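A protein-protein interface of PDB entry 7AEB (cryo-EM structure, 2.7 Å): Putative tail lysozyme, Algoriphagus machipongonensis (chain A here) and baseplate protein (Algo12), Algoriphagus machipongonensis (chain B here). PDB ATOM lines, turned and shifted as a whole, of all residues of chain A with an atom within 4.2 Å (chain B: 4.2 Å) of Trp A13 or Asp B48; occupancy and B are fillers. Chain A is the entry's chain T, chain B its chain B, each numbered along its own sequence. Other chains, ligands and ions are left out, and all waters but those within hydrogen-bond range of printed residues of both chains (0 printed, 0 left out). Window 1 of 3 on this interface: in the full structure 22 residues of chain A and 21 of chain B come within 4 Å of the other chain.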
ATOM      1  N   GLY A  12     -15.444 -16.351 -26.869  1.00  0.00           N
ATOM      2  CA  GLY A  12     -14.502 -17.231 -26.182  1.00  0.00           C
ATOM      3  C   GLY A  12     -14.072 -16.719 -24.818  1.00  0.00           C
ATOM      4  O   GLY A  12     -14.597 -15.737 -24.331  1.00  0.00           O
ATOM      5  N   TRP A  13     -13.094 -17.389 -24.210  1.00  0.00           N
ATOM      6  CA  TRP A  13     -12.617 -17.038 -22.871  1.00  0.00           C
ATOM      7  C   TRP A  13     -11.849 -15.721 -22.882  1.00  0.00           C
ATOM      8  O   TRP A  13     -11.117 -15.443 -23.827  1.00  0.00           O
ATOM      9  CB  TRP A  13     -11.676 -18.120 -22.349  1.00  0.00           C
ATOM     10  CG  TRP A  13     -12.269 -19.464 -22.012  1.00  0.00           C
ATOM     11  CD1 TRP A  13     -13.059 -20.247 -22.806  1.00  0.00           C
ATOM     12  CD2 TRP A  13     -12.077 -20.194 -20.800  1.00  0.00           C
ATOM     13  NE1 TRP A  13     -13.373 -21.406 -22.152  1.00  0.00           N
ATOM     14  CE2 TRP A  13     -12.782 -21.393 -20.920  1.00  0.00           C
ATOM     15  CE3 TRP A  13     -11.380 -19.941 -19.619  1.00  0.00           C
ATOM     16  CZ2 TRP A  13     -12.813 -22.331 -19.909  1.00  0.00           C
ATOM     17  CZ3 TRP A  13     -11.412 -20.877 -18.621  1.00  0.00           C
ATOM     18  CH2 TRP A  13     -12.119 -22.050 -18.768  1.00  0.00           C
ATOM     19  N   GLY A  14     -11.979 -14.913 -21.826  1.00  0.00           N
ATOM     20  CA  GLY A  14     -11.159 -13.705 -21.733  1.00  0.00           C
ATOM     21  C   GLY A  14      -9.705 -14.086 -21.516  1.00  0.00           C
ATOM     22  O   GLY A  14      -9.428 -15.130 -20.953  1.00  0.00           O
ATOM     23  N   PHE A  15      -8.718 -13.286 -21.960  1.00  0.00           N
ATOM     24  CA  PHE A  15      -7.347 -13.789 -21.800  1.00  0.00           C
ATOM     25  C   PHE A  15      -6.889 -13.908 -20.368  1.00  0.00           C
ATOM     26  O   PHE A  15      -6.368 -14.973 -20.022  1.00  0.00           O
ATOM     27  CB  PHE A  15      -6.323 -12.980 -22.594  1.00  0.00           C
ATOM     28  CG  PHE A  15      -4.913 -13.101 -22.034  1.00  0.00           C
ATOM     29  CD1 PHE A  15      -4.293 -14.344 -21.816  1.00  0.00           C
ATOM     30  CD2 PHE A  15      -4.143 -11.982 -21.863  1.00  0.00           C
ATOM     31  CE1 PHE A  15      -3.084 -14.454 -21.281  1.00  0.00           C
ATOM     32  CE2 PHE A  15      -2.857 -12.096 -21.395  1.00  0.00           C
ATOM     33  CZ  PHE A  15      -2.331 -13.334 -21.112  1.00  0.00           C
ATOM     34  N   VAL A  26     -16.908 -18.159 -15.649  1.00  0.00           N
ATOM     35  CA  VAL A  26     -15.692 -17.504 -16.110  1.00  0.00           C
ATOM     36  C   VAL A  26     -16.110 -16.510 -17.179  1.00  0.00           C
ATOM     37  O   VAL A  26     -16.978 -16.805 -18.008  1.00  0.00           O
ATOM     38  CB  VAL A  26     -14.643 -18.514 -16.638  1.00  0.00           C
ATOM     39  CG1 VAL A  26     -15.113 -19.253 -17.898  1.00  0.00           C
ATOM     40  CG2 VAL A  26     -13.308 -17.820 -16.896  1.00  0.00           C
ATOM     41  N   LYS A  27     -15.549 -15.311 -17.125  1.00  0.00           N
ATOM     42  CA  LYS A  27     -15.913 -14.285 -18.090  1.00  0.00           C
ATOM     43  C   LYS A  27     -15.441 -14.608 -19.497  1.00  0.00           C
ATOM     44  O   LYS A  27     -14.340 -15.127 -19.712  1.00  0.00           O
ATOM     45  CB  LYS A  27     -15.325 -12.945 -17.696  1.00  0.00           C
ATOM     46  CG  LYS A  27     -15.905 -12.352 -16.468  1.00  0.00           C
ATOM     47  CD  LYS A  27     -15.321 -10.982 -16.243  1.00  0.00           C
ATOM     48  CE  LYS A  27     -15.827 -10.389 -14.960  1.00  0.00           C
ATOM     49  NZ  LYS A  27     -15.252  -9.055 -14.706  1.00  0.00           N
ATOM     50  N   THR A  29     -15.511 -13.087 -23.834  1.00  0.00           N
ATOM     51  CA  THR A  29     -15.403 -11.955 -24.749  1.00  0.00           C
ATOM     52  C   THR A  29     -16.008 -12.313 -26.103  1.00  0.00           C
ATOM     53  O   THR A  29     -16.189 -13.482 -26.431  1.00  0.00           O
ATOM     54  CB  THR A  29     -13.925 -11.518 -24.909  1.00  0.00           C
ATOM     55  OG1 THR A  29     -13.118 -12.608 -25.394  1.00  0.00           O
ATOM     56  CG2 THR A  29     -13.373 -11.046 -23.590  1.00  0.00           C
ATOM     57  N   TRP B  41     -19.628 -21.284 -26.266  1.00  0.00           N
ATOM     58  CA  TRP B  41     -18.231 -21.293 -26.651  1.00  0.00           C
ATOM     59  C   TRP B  41     -18.105 -21.753 -28.089  1.00  0.00           C
ATOM     60  O   TRP B  41     -18.193 -22.949 -28.359  1.00  0.00           O
ATOM     61  CB  TRP B  41     -17.465 -22.206 -25.715  1.00  0.00           C
ATOM     62  CG  TRP B  41     -16.004 -22.289 -25.916  1.00  0.00           C
ATOM     63  CD1 TRP B  41     -15.205 -21.489 -26.639  1.00  0.00           C
ATOM     64  CD2 TRP B  41     -15.157 -23.254 -25.334  1.00  0.00           C
ATOM     65  NE1 TRP B  41     -13.924 -21.904 -26.551  1.00  0.00           N
ATOM     66  CE2 TRP B  41     -13.878 -22.992 -25.763  1.00  0.00           C
ATOM     67  CE3 TRP B  41     -15.363 -24.317 -24.482  1.00  0.00           C
ATOM     68  CZ2 TRP B  41     -12.825 -23.739 -25.398  1.00  0.00           C
ATOM     69  CZ3 TRP B  41     -14.296 -25.064 -24.103  1.00  0.00           C
ATOM     70  CH2 TRP B  41     -13.053 -24.779 -24.555  1.00  0.00           C
ATOM     71  N   ASP B  43     -15.582 -20.003 -30.426  1.00  0.00           N
ATOM     72  CA  ASP B  43     -14.290 -19.612 -30.964  1.00  0.00           C
ATOM     73  C   ASP B  43     -13.274 -20.693 -30.623  1.00  0.00           C
ATOM     74  O   ASP B  43     -12.807 -20.742 -29.500  1.00  0.00           O
ATOM     75  CB  ASP B  43     -13.942 -18.281 -30.304  1.00  0.00           C
ATOM     76  CG  ASP B  43     -12.556 -17.794 -30.588  1.00  0.00           C
ATOM     77  OD1 ASP B  43     -11.729 -18.494 -31.143  1.00  0.00           O
ATOM     78  OD2 ASP B  43     -12.242 -16.667 -30.216  1.00  0.00           O
ATOM     79  N   ASN B  45     -10.182 -21.019 -32.082  1.00  0.00           N
ATOM     80  CA  ASN B  45      -8.890 -20.622 -32.605  1.00  0.00           C
ATOM     81  C   ASN B  45      -7.783 -20.838 -31.590  1.00  0.00           C
ATOM     82  O   ASN B  45      -8.014 -20.917 -30.389  1.00  0.00           O
ATOM     83  CB  ASN B  45      -8.922 -19.181 -33.023  1.00  0.00           C
ATOM     84  CG  ASN B  45      -9.622 -18.991 -34.269  1.00  0.00           C
ATOM     85  OD1 ASN B  45      -9.139 -19.408 -35.316  1.00  0.00           O
ATOM     86  ND2 ASN B  45     -10.764 -18.383 -34.202  1.00  0.00           N
ATOM     87  N   THR B  46      -6.553 -20.872 -32.082  1.00  0.00           N
ATOM     88  CA  THR B  46      -5.408 -21.209 -31.248  1.00  0.00           C
ATOM     89  C   THR B  46      -5.018 -20.158 -30.203  1.00  0.00           C
ATOM     90  O   THR B  46      -4.249 -20.475 -29.301  1.00  0.00           O
ATOM     91  CB  THR B  46      -4.185 -21.456 -32.113  1.00  0.00           C
ATOM     92  OG1 THR B  46      -3.968 -20.342 -32.970  1.00  0.00           O
ATOM     93  CG2 THR B  46      -4.458 -22.667 -32.980  1.00  0.00           C
ATOM     94  N   HIS B  47      -5.517 -18.936 -30.274  1.00  0.00           N
ATOM     95  CA  HIS B  47      -5.179 -17.976 -29.235  1.00  0.00           C
ATOM     96  C   HIS B  47      -6.051 -18.141 -28.000  1.00  0.00           C
ATOM     97  O   HIS B  47      -5.824 -17.460 -26.999  1.00  0.00           O
ATOM     98  CB  HIS B  47      -5.356 -16.561 -29.724  1.00  0.00           C
ATOM     99  CG  HIS B  47      -6.757 -16.237 -29.950  1.00  0.00           C
ATOM    100  ND1 HIS B  47      -7.442 -16.681 -31.042  1.00  0.00           N
ATOM    101  CD2 HIS B  47      -7.631 -15.553 -29.198  1.00  0.00           C
ATOM    102  CE1 HIS B  47      -8.688 -16.265 -30.959  1.00  0.00           C
ATOM    103  NE2 HIS B  47      -8.828 -15.580 -29.848  1.00  0.00           N
ATOM    104  N   ASP B  48      -7.070 -18.985 -28.079  1.00  0.00           N
ATOM    105  CA  ASP B  48      -8.059 -19.180 -27.023  1.00  0.00           C
ATOM    106  C   ASP B  48      -7.509 -19.961 -25.827  1.00  0.00           C
ATOM    107  O   ASP B  48      -7.018 -21.070 -26.013  1.00  0.00           O
ATOM    108  CB  ASP B  48      -9.272 -19.918 -27.583  1.00  0.00           C
ATOM    109  CG  ASP B  48     -10.380 -20.110 -26.549  1.00  0.00           C
ATOM    110  OD1 ASP B  48     -10.220 -19.736 -25.405  1.00  0.00           O
ATOM    111  OD2 ASP B  48     -11.395 -20.679 -26.872  1.00  0.00           O
ATOM    112  N   PRO B  49      -7.532 -19.389 -24.605  1.00  0.00           N
ATOM    113  CA  PRO B  49      -7.122 -20.066 -23.374  1.00  0.00           C
ATOM    114  C   PRO B  49      -7.780 -21.419 -23.184  1.00  0.00           C
ATOM    115  O   PRO B  49      -7.150 -22.340 -22.665  1.00  0.00           O
ATOM    116  CB  PRO B  49      -7.577 -19.073 -22.306  1.00  0.00           C
ATOM    117  CG  PRO B  49      -7.491 -17.750 -22.983  1.00  0.00           C
ATOM    118  CD  PRO B  49      -7.916 -17.991 -24.386  1.00  0.00           C
ATOM    119  N   GLY B  50      -9.026 -21.565 -23.632  1.00  0.00           N
ATOM    120  CA  GLY B  50      -9.744 -22.817 -23.526  1.00  0.00           C
ATOM    121  C   GLY B  50      -9.031 -23.929 -24.260  1.00  0.00           C
ATOM    122  O   GLY B  50      -8.742 -24.990 -23.701  1.00  0.00           O
ATOM    123  N   ILE B  51      -8.761 -23.672 -25.531  1.00  0.00           N
ATOM    124  CA  ILE B  51      -8.073 -24.619 -26.389  1.00  0.00           C
ATOM    125  C   ILE B  51      -6.667 -24.879 -25.869  1.00  0.00           C
ATOM    126  O   ILE B  51      -6.181 -26.010 -25.940  1.00  0.00           O
ATOM    127  CB  ILE B  51      -8.062 -24.120 -27.848  1.00  0.00           C
ATOM    128  CG1 ILE B  51      -9.511 -24.004 -28.403  1.00  0.00           C
ATOM    129  CG2 ILE B  51      -7.201 -25.029 -28.741  1.00  0.00           C
ATOM    130  CD1 ILE B  51     -10.366 -25.281 -28.429  1.00  0.00           C
ATOM    131  N   THR B  52      -5.987 -23.843 -25.373  1.00  0.00           N
ATOM    132  CA  THR B  52      -4.650 -24.032 -24.818  1.00  0.00           C
ATOM    133  C   THR B  52      -4.669 -25.059 -23.690  1.00  0.00           C
ATOM    134  O   THR B  52      -3.836 -25.970 -23.657  1.00  0.00           O
ATOM    135  CB  THR B  52      -4.079 -22.702 -24.304  1.00  0.00           C
ATOM    136  OG1 THR B  52      -3.945 -21.781 -25.389  1.00  0.00           O
ATOM    137  CG2 THR B  52      -2.721 -22.902 -23.651  1.00  0.00           C
ATOM    138  N   TYR B 425      -8.128 -23.043  -9.975  1.00  0.00           N
ATOM    139  CA  TYR B 425      -8.898 -23.804 -10.950  1.00  0.00           C
ATOM    140  C   TYR B 425      -8.129 -25.003 -11.467  1.00  0.00           C
ATOM    141  O   TYR B 425      -8.643 -26.120 -11.486  1.00  0.00           O
ATOM    142  CB  TYR B 425      -9.298 -22.888 -12.096  1.00  0.00           C
ATOM    143  CG  TYR B 425     -10.035 -23.542 -13.218  1.00  0.00           C
ATOM    144  CD1 TYR B 425     -11.353 -23.883 -13.071  1.00  0.00           C
ATOM    145  CD2 TYR B 425      -9.415 -23.767 -14.424  1.00  0.00           C
ATOM    146  CE1 TYR B 425     -12.036 -24.451 -14.097  1.00  0.00           C
ATOM    147  CE2 TYR B 425     -10.099 -24.330 -15.454  1.00  0.00           C
ATOM    148  CZ  TYR B 425     -11.408 -24.670 -15.286  1.00  0.00           C
ATOM    149  OH  TYR B 425     -12.100 -25.241 -16.317  1.00  0.00           O
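O of Asp B43 is in hydrogen-bond range of NE1 of Trp B41 (3.4 Å).
NE1 of Trp B41 lies within hydrogen-bond range of OD2 of Asp B48 (2.8 Å).
N of Gly B50 lies within hydrogen-bond range of OD1 of Asp B48, at 2.8 Å.
The backbone carbonyl oxygen (O) of Asp B48 is in hydrogen-bond range of the side-chain hydroxyl (OG1) of Thr B52 (3.2 Å).
O of Lys A27 sits at hydrogen-bond distance from N of Gly A14.
Trp B41 touches Trp A13.
Asp B48 touches Trp A13.
Gly A14 touches Pro B49.
Printed residues of chain A within 4 Å of Trp B41: Trp A13.
Asp B48 touches just one residue of chain A: Trp A13 (3.8 Å).
Of the printed residues of chain A, Pro B49 touches Gly A14.
Of the 7 printed residues of chain A, 2 touch a printed residue of chain B.
Printed residues of chain A that touch a printed residue of chain B: Trp A13 and Gly A14.
Hydrophobic or aromatic side chains of chain A that line the printed part of chain B: Trp A13.
Of the 11 printed residues of chain B, 3 touch a printed residue of chain A.
Among the printed residues, no Asp or Glu carboxylate lies within 4 Å of a Lys or Arg side-chain nitrogen of the other chain.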
